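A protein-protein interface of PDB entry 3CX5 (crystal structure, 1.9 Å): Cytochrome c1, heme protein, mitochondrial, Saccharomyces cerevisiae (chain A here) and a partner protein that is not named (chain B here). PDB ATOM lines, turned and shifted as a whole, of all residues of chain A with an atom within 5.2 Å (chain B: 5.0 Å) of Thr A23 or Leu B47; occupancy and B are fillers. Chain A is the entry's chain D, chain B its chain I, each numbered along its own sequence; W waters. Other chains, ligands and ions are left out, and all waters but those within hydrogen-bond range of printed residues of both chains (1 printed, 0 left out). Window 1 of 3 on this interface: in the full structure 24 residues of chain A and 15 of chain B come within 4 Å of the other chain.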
ATOM      1  N   SER A  16       7.206 -14.890  -4.296  1.00  0.00           N
ATOM      2  CA  SER A  16       6.564 -13.804  -3.572  1.00  0.00           C
ATOM      3  C   SER A  16       5.207 -13.402  -4.144  1.00  0.00           C
ATOM      4  O   SER A  16       4.500 -12.593  -3.546  1.00  0.00           O
ATOM      5  CB  SER A  16       7.498 -12.593  -3.448  1.00  0.00           C
ATOM      6  OG  SER A  16       7.907 -12.109  -4.712  1.00  0.00           O
ATOM      7  N   HIS A  17       4.851 -13.953  -5.303  1.00  0.00           N
ATOM      8  CA  HIS A  17       3.552 -13.665  -5.907  1.00  0.00           C
ATOM      9  C   HIS A  17       2.530 -14.788  -5.630  1.00  0.00           C
ATOM     10  O   HIS A  17       1.370 -14.690  -6.031  1.00  0.00           O
ATOM     11  CB  HIS A  17       3.674 -13.336  -7.408  1.00  0.00           C
ATOM     12  CG  HIS A  17       4.505 -14.310  -8.188  1.00  0.00           C
ATOM     13  ND1 HIS A  17       3.991 -15.475  -8.716  1.00  0.00           N
ATOM     14  CD2 HIS A  17       5.809 -14.279  -8.550  1.00  0.00           C
ATOM     15  CE1 HIS A  17       4.942 -16.119  -9.370  1.00  0.00           C
ATOM     16  NE2 HIS A  17       6.055 -15.414  -9.284  1.00  0.00           N
ATOM     17  N   PHE A  21      -3.282 -12.440  -1.901  1.00  0.00           N
ATOM     18  CA  PHE A  21      -3.061 -11.006  -1.717  1.00  0.00           C
ATOM     19  C   PHE A  21      -1.723 -10.495  -2.254  1.00  0.00           C
ATOM     20  O   PHE A  21      -1.407  -9.318  -2.093  1.00  0.00           O
ATOM     21  CB  PHE A  21      -3.166 -10.651  -0.231  1.00  0.00           C
ATOM     22  CG  PHE A  21      -4.363 -11.243   0.462  1.00  0.00           C
ATOM     23  CD1 PHE A  21      -4.199 -12.059   1.579  1.00  0.00           C
ATOM     24  CD2 PHE A  21      -5.651 -10.989   0.000  1.00  0.00           C
ATOM     25  CE1 PHE A  21      -5.301 -12.612   2.228  1.00  0.00           C
ATOM     26  CE2 PHE A  21      -6.759 -11.535   0.639  1.00  0.00           C
ATOM     27  CZ  PHE A  21      -6.590 -12.349   1.756  1.00  0.00           C
ATOM     28  N   GLU A  22      -0.970 -11.348  -2.941  1.00  0.00           N
ATOM     29  CA  GLU A  22       0.354 -10.955  -3.427  1.00  0.00           C
ATOM     30  C   GLU A  22       0.523 -10.523  -4.881  1.00  0.00           C
ATOM     31  O   GLU A  22       0.108 -11.225  -5.808  1.00  0.00           O
ATOM     32  CB  GLU A  22       1.366 -12.072  -3.148  1.00  0.00           C
ATOM     33  CG  GLU A  22       1.302 -12.681  -1.748  1.00  0.00           C
ATOM     34  CD  GLU A  22       1.378 -11.651  -0.640  1.00  0.00           C
ATOM     35  OE1 GLU A  22       0.644 -11.815   0.358  1.00  0.00           O
ATOM     36  OE2 GLU A  22       2.156 -10.684  -0.761  1.00  0.00           O
ATOM     37  N   THR A  23       1.182  -9.384  -5.069  1.00  0.00           N
ATOM     38  CA  THR A  23       1.481  -8.881  -6.408  1.00  0.00           C
ATOM     39  C   THR A  23       2.854  -9.433  -6.798  1.00  0.00           C
ATOM     40  O   THR A  23       3.544 -10.052  -5.978  1.00  0.00           O
ATOM     41  CB  THR A  23       1.613  -7.336  -6.448  1.00  0.00           C
ATOM     42  OG1 THR A  23       2.761  -6.931  -5.689  1.00  0.00           O
ATOM     43  CG2 THR A  23       0.373  -6.662  -5.895  1.00  0.00           C
ATOM     44  N   PHE A  24       3.239  -9.216  -8.051  1.00  0.00           N
ATOM     45  CA  PHE A  24       4.551  -9.636  -8.532  1.00  0.00           C
ATOM     46  C   PHE A  24       5.569  -8.702  -7.881  1.00  0.00           C
ATOM     47  O   PHE A  24       5.224  -7.587  -7.466  1.00  0.00           O
ATOM     48  CB  PHE A  24       4.686  -9.407 -10.044  1.00  0.00           C
ATOM     49  CG  PHE A  24       4.040 -10.458 -10.907  1.00  0.00           C
ATOM     50  CD1 PHE A  24       3.220 -10.086 -11.970  1.00  0.00           C
ATOM     51  CD2 PHE A  24       4.282 -11.806 -10.696  1.00  0.00           C
ATOM     52  CE1 PHE A  24       2.654 -11.045 -12.805  1.00  0.00           C
ATOM     53  CE2 PHE A  24       3.716 -12.772 -11.528  1.00  0.00           C
ATOM     54  CZ  PHE A  24       2.902 -12.389 -12.582  1.00  0.00           C
ATOM     55  N   ASP A  25       6.811  -9.167  -7.776  1.00  0.00           N
ATOM     56  CA  ASP A  25       7.895  -8.330  -7.270  1.00  0.00           C
ATOM     57  C   ASP A  25       8.401  -7.670  -8.555  1.00  0.00           C
ATOM     58  O   ASP A  25       9.054  -8.314  -9.379  1.00  0.00           O
ATOM     59  CB  ASP A  25       9.007  -9.179  -6.641  1.00  0.00           C
ATOM     60  CG  ASP A  25      10.154  -8.334  -6.078  1.00  0.00           C
ATOM     61  OD1 ASP A  25      10.772  -8.763  -5.083  1.00  0.00           O
ATOM     62  OD2 ASP A  25      10.448  -7.248  -6.618  1.00  0.00           O
ATOM     63  N   HIS A  26       8.092  -6.391  -8.728  1.00  0.00           N
ATOM     64  CA  HIS A  26       8.486  -5.680  -9.935  1.00  0.00           C
ATOM     65  C   HIS A  26       9.979  -5.445 -10.144  1.00  0.00           C
ATOM     66  O   HIS A  26      10.418  -5.229 -11.275  1.00  0.00           O
ATOM     67  CB  HIS A  26       7.669  -4.400 -10.090  1.00  0.00           C
ATOM     68  CG  HIS A  26       6.222  -4.658 -10.374  1.00  0.00           C
ATOM     69  ND1 HIS A  26       5.637  -4.356 -11.583  1.00  0.00           N
ATOM     70  CD2 HIS A  26       5.261  -5.257  -9.630  1.00  0.00           C
ATOM     71  CE1 HIS A  26       4.380  -4.763 -11.575  1.00  0.00           C
ATOM     72  NE2 HIS A  26       4.127  -5.312 -10.403  1.00  0.00           N
ATOM     73  N   HIS A 202      -2.253 -10.004 -13.797  1.00  0.00           N
ATOM     74  CA  HIS A 202      -2.026 -10.587 -12.464  1.00  0.00           C
ATOM     75  C   HIS A 202      -2.306  -9.702 -11.248  1.00  0.00           C
ATOM     76  O   HIS A 202      -3.157 -10.031 -10.426  1.00  0.00           O
ATOM     77  CB  HIS A 202      -0.591 -11.120 -12.389  1.00  0.00           C
ATOM     78  CG  HIS A 202      -0.250 -11.788 -11.094  1.00  0.00           C
ATOM     79  ND1 HIS A 202       0.244 -11.099 -10.007  1.00  0.00           N
ATOM     80  CD2 HIS A 202      -0.316 -13.087 -10.719  1.00  0.00           C
ATOM     81  CE1 HIS A 202       0.467 -11.944  -9.018  1.00  0.00           C
ATOM     82  NE2 HIS A 202       0.136 -13.157  -9.423  1.00  0.00           N
ATOM     83  N   ASP A 203      -1.579  -8.593 -11.129  1.00  0.00           N
ATOM     84  CA  ASP A 203      -1.743  -7.687  -9.993  1.00  0.00           C
ATOM     85  C   ASP A 203      -3.132  -7.071  -9.879  1.00  0.00           C
ATOM     86  O   ASP A 203      -3.696  -6.998  -8.783  1.00  0.00           O
ATOM     87  CB  ASP A 203      -0.680  -6.588 -10.032  1.00  0.00           C
ATOM     88  CG  ASP A 203       0.737  -7.124  -9.837  1.00  0.00           C
ATOM     89  OD1 ASP A 203       0.922  -8.345  -9.615  1.00  0.00           O
ATOM     90  OD2 ASP A 203       1.677  -6.313  -9.910  1.00  0.00           O
ATOM     91  N   TYR B  39      -4.276  -3.039  -0.170  1.00  0.00           N
ATOM     92  CA  TYR B  39      -3.607  -3.918  -1.120  1.00  0.00           C
ATOM     93  C   TYR B  39      -2.196  -3.436  -1.457  1.00  0.00           C
ATOM     94  O   TYR B  39      -1.241  -4.224  -1.437  1.00  0.00           O
ATOM     95  CB  TYR B  39      -4.456  -4.032  -2.390  1.00  0.00           C
ATOM     96  CG  TYR B  39      -3.963  -5.044  -3.401  1.00  0.00           C
ATOM     97  CD1 TYR B  39      -4.048  -6.417  -3.146  1.00  0.00           C
ATOM     98  CD2 TYR B  39      -3.453  -4.630  -4.632  1.00  0.00           C
ATOM     99  CE1 TYR B  39      -3.637  -7.356  -4.100  1.00  0.00           C
ATOM    100  CE2 TYR B  39      -3.040  -5.558  -5.592  1.00  0.00           C
ATOM    101  CZ  TYR B  39      -3.135  -6.915  -5.319  1.00  0.00           C
ATOM    102  OH  TYR B  39      -2.722  -7.825  -6.268  1.00  0.00           O
ATOM    103  N   GLU B  40      -2.071  -2.149  -1.774  1.00  0.00           N
ATOM    104  CA  GLU B  40      -0.773  -1.569  -2.109  1.00  0.00           C
ATOM    105  C   GLU B  40       0.172  -1.558  -0.908  1.00  0.00           C
ATOM    106  O   GLU B  40       1.374  -1.773  -1.057  1.00  0.00           O
ATOM    107  CB  GLU B  40      -0.940  -0.160  -2.684  1.00  0.00           C
ATOM    108  CG  GLU B  40      -1.532  -0.158  -4.094  1.00  0.00           C
ATOM    109  CD  GLU B  40      -1.631   1.224  -4.721  1.00  0.00           C
ATOM    110  OE1 GLU B  40      -1.971   1.294  -5.922  1.00  0.00           O
ATOM    111  OE2 GLU B  40      -1.377   2.236  -4.028  1.00  0.00           O
ATOM    112  N   ASN B  43       1.647  -4.980  -0.242  1.00  0.00           N
ATOM    113  CA  ASN B  43       2.688  -5.333  -1.197  1.00  0.00           C
ATOM    114  C   ASN B  43       3.784  -4.276  -1.335  1.00  0.00           C
ATOM    115  O   ASN B  43       4.518  -4.260  -2.327  1.00  0.00           O
ATOM    116  CB  ASN B  43       2.050  -5.618  -2.556  1.00  0.00           C
ATOM    117  CG  ASN B  43       1.203  -6.871  -2.538  1.00  0.00           C
ATOM    118  OD1 ASN B  43       1.728  -7.977  -2.592  1.00  0.00           O
ATOM    119  ND2 ASN B  43      -0.113  -6.703  -2.439  1.00  0.00           N
ATOM    120  N   GLY B  45       7.020  -2.244  -1.494  1.00  0.00           N
ATOM    121  CA  GLY B  45       8.361  -2.676  -1.832  1.00  0.00           C
ATOM    122  C   GLY B  45       8.387  -3.445  -3.140  1.00  0.00           C
ATOM    123  O   GLY B  45       9.397  -3.445  -3.844  1.00  0.00           O
ATOM    124  N   LYS B  46       7.268  -4.083  -3.476  1.00  0.00           N
ATOM    125  CA  LYS B  46       7.155  -4.874  -4.704  1.00  0.00           C
ATOM    126  C   LYS B  46       6.594  -4.096  -5.895  1.00  0.00           C
ATOM    127  O   LYS B  46       6.898  -4.408  -7.045  1.00  0.00           O
ATOM    128  CB  LYS B  46       6.300  -6.116  -4.442  1.00  0.00           C
ATOM    129  CG  LYS B  46       6.988  -7.167  -3.590  1.00  0.00           C
ATOM    130  CD  LYS B  46       5.989  -7.998  -2.801  1.00  0.00           C
ATOM    131  CE  LYS B  46       5.017  -8.748  -3.692  1.00  0.00           C
ATOM    132  NZ  LYS B  46       4.063  -9.572  -2.892  1.00  0.00           N
ATOM    133  N   LEU B  47       5.771  -3.093  -5.610  1.00  0.00           N
ATOM    134  CA  LEU B  47       5.146  -2.271  -6.642  1.00  0.00           C
ATOM    135  C   LEU B  47       6.158  -1.477  -7.446  1.00  0.00           C
ATOM    136  O   LEU B  47       7.219  -1.121  -6.934  1.00  0.00           O
ATOM    137  CB  LEU B  47       4.137  -1.311  -6.007  1.00  0.00           C
ATOM    138  CG  LEU B  47       2.719  -1.817  -5.732  1.00  0.00           C
ATOM    139  CD1 LEU B  47       2.722  -3.250  -5.240  1.00  0.00           C
ATOM    140  CD2 LEU B  47       2.044  -0.893  -4.731  1.00  0.00           C
ATOM    141  N   TRP B  48       5.827  -1.217  -8.709  1.00  0.00           N
ATOM    142  CA  TRP B  48       6.696  -0.446  -9.591  1.00  0.00           C
ATOM    143  C   TRP B  48       6.995   0.938  -9.011  1.00  0.00           C
ATOM    144  O   TRP B  48       8.112   1.431  -9.141  1.00  0.00           O
ATOM    145  CB  TRP B  48       6.071  -0.304 -10.986  1.00  0.00           C
ATOM    146  CG  TRP B  48       6.796   0.680 -11.874  1.00  0.00           C
ATOM    147  CD1 TRP B  48       6.288   1.831 -12.405  1.00  0.00           C
ATOM    148  CD2 TRP B  48       8.161   0.610 -12.305  1.00  0.00           C
ATOM    149  NE1 TRP B  48       7.249   2.481 -13.140  1.00  0.00           N
ATOM    150  CE2 TRP B  48       8.409   1.755 -13.095  1.00  0.00           C
ATOM    151  CE3 TRP B  48       9.202  -0.305 -12.097  1.00  0.00           C
ATOM    152  CZ2 TRP B  48       9.657   2.011 -13.681  1.00  0.00           C
ATOM    153  CZ3 TRP B  48      10.446  -0.050 -12.679  1.00  0.00           C
ATOM    154  CH2 TRP B  48      10.658   1.100 -13.463  1.00  0.00           C
ATOM    155  N   LYS B  49       5.999   1.556  -8.380  1.00  0.00           N
ATOM    156  CA  LYS B  49       6.170   2.883  -7.778  1.00  0.00           C
ATOM    157  C   LYS B  49       7.309   2.837  -6.771  1.00  0.00           C
ATOM    158  O   LYS B  49       8.146   3.738  -6.718  1.00  0.00           O
ATOM    159  CB  LYS B  49       4.917   3.319  -7.019  1.00  0.00           C
ATOM    160  CG  LYS B  49       3.620   3.296  -7.787  1.00  0.00           C
ATOM    161  CD  LYS B  49       2.494   3.839  -6.907  1.00  0.00           C
ATOM    162  CE  LYS B  49       2.469   3.146  -5.546  1.00  0.00           C
ATOM    163  NZ  LYS B  49       1.412   3.694  -4.649  1.00  0.00           N
ATOM    164  N   ASP B  50       7.305   1.784  -5.957  1.00  0.00           N
ATOM    165  CA  ASP B  50       8.315   1.586  -4.929  1.00  0.00           C
ATOM    166  C   ASP B  50       9.682   1.307  -5.552  1.00  0.00           C
ATOM    167  O   ASP B  50      10.697   1.820  -5.085  1.00  0.00           O
ATOM    168  CB  ASP B  50       7.903   0.432  -4.006  1.00  0.00           C
ATOM    169  CG  ASP B  50       6.490   0.594  -3.448  1.00  0.00           C
ATOM    170  OD1 ASP B  50       5.813  -0.435  -3.243  1.00  0.00           O
ATOM    171  OD2 ASP B  50       6.051   1.741  -3.206  1.00  0.00           O
ATOM    172  N   VAL B  51       9.698   0.521  -6.627  1.00  0.00           N
ATOM    173  CA  VAL B  51      10.940   0.176  -7.312  1.00  0.00           C
ATOM    174  C   VAL B  51      11.520   1.385  -8.039  1.00  0.00           C
ATOM    175  O   VAL B  51      12.731   1.598  -8.031  1.00  0.00           O
ATOM    176  CB  VAL B  51      10.732  -0.982  -8.322  1.00  0.00           C
ATOM    177  CG1 VAL B  51      12.045  -1.328  -9.015  1.00  0.00           C
ATOM    178  CG2 VAL B  51      10.179  -2.208  -7.612  1.00  0.00           C
HETATM  179  O   HOH W   1       5.529 -10.984  -0.989  1.00  0.00           O
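O of Ser A16 lies within hydrogen-bond range of NZ of Lys B46, 3.1 Å away.
N of Thr A23 sits at hydrogen-bond distance from OD1 of Asn B43, 2.9 Å away.
The side-chain amino group (NZ) of Lys B46 is in salt-bridge range of the side-chain carboxylate (OE2) of Glu A22.
The backbone carbonyl oxygen of Thr A23 sits close to the side-chain amino group of Lys B46 (3.2 Å).
The side-chain hydroxyl (OH) of Tyr B39 sits at hydrogen-bond distance from the backbone carbonyl oxygen (O) of Asp A203.
OD1 of Asn B43 lies close to OE2 of Glu A22 (3.3 Å).
The backbone NH (N) of His A26 lies within hydrogen-bond range of the backbone carbonyl oxygen (O) of Lys B46, at 2.9 Å.
The side-chain amide nitrogen of Asn B43 is in hydrogen-bond range of the backbone carbonyl oxygen of Phe A21 (2.9 Å).
The side-chain amide nitrogen of Asn B43 is in hydrogen-bond range of the backbone carbonyl oxygen of Tyr B39, 2.9 Å away.
The side-chain carboxylate (OD1) of Asp A203 lies within hydrogen-bond range of a ring nitrogen (ND1) of His A202.
The side-chain carboxylate (OD1) of Asp A203 lies within hydrogen-bond range of the backbone NH (N) of Phe A24 (2.9 Å).
The side-chain carboxylate of Asp A203 lies within hydrogen-bond range of a ring nitrogen (NE2) of His A26, 2.7 Å away.
The side-chain amide oxygen of Asn B43 is in hydrogen-bond range of the side-chain amino group of Lys B46 (2.8 Å).
Tyr B39 touches Phe A21.
CG2 of Thr A23 touches OH of Tyr B39, at 3.3 Å.
Leu B47 touches Thr A23 (CD1 to OG1, 3.7 Å).
Lys B46 touches Phe A24 (CB to O, 3.5 Å).
Asp A25 touches Lys B46 (C to O, 3.9 Å).
CG of His A26 touches N of Trp B48 (3.8 Å).
Printed residues of chain B within 4 Å of Phe A21: Tyr B39 (3.6 Å) and Asn B43 (2.9 Å).
Thr A23 touches just these residues of chain B: Tyr B39, Asn B43, Lys B46 and Leu B47.
Of the printed residues of chain B, His A26 touches Lys B46 (2.9 Å) and Trp B48 (3.8 Å).
His A202 touches none of the printed residues of chain B.
Of the printed residues of chain B, Asp A203 touches Tyr B39.
The nearest residue of chain A that does not touch Leu B47 is His A26 (4.2 Å).
Printed residues of chain B that touch a printed residue of chain A: Tyr B39, Asn B43, Lys B46, Leu B47 and Trp B48.
Hydrophobic or aromatic side chains of chain B within 4 Å of the printed part of chain A: Tyr B39 and Leu B47.
Along chain B the printed residues that touch a printed residue of chain A span positions 39 to 48.
Among the printed residues, Asp or Glu carboxylates within 4 Å of a Lys or Arg side-chain nitrogen of the other chain: Glu A22 with Lys B46 (3.1 Å).
Water W1 lies within hydrogen-bond range of NZ of Lys B46 (2.8 Å), O of Ser A16 (3.2 Å) and OE2 of Glu A22 (3.4 Å).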
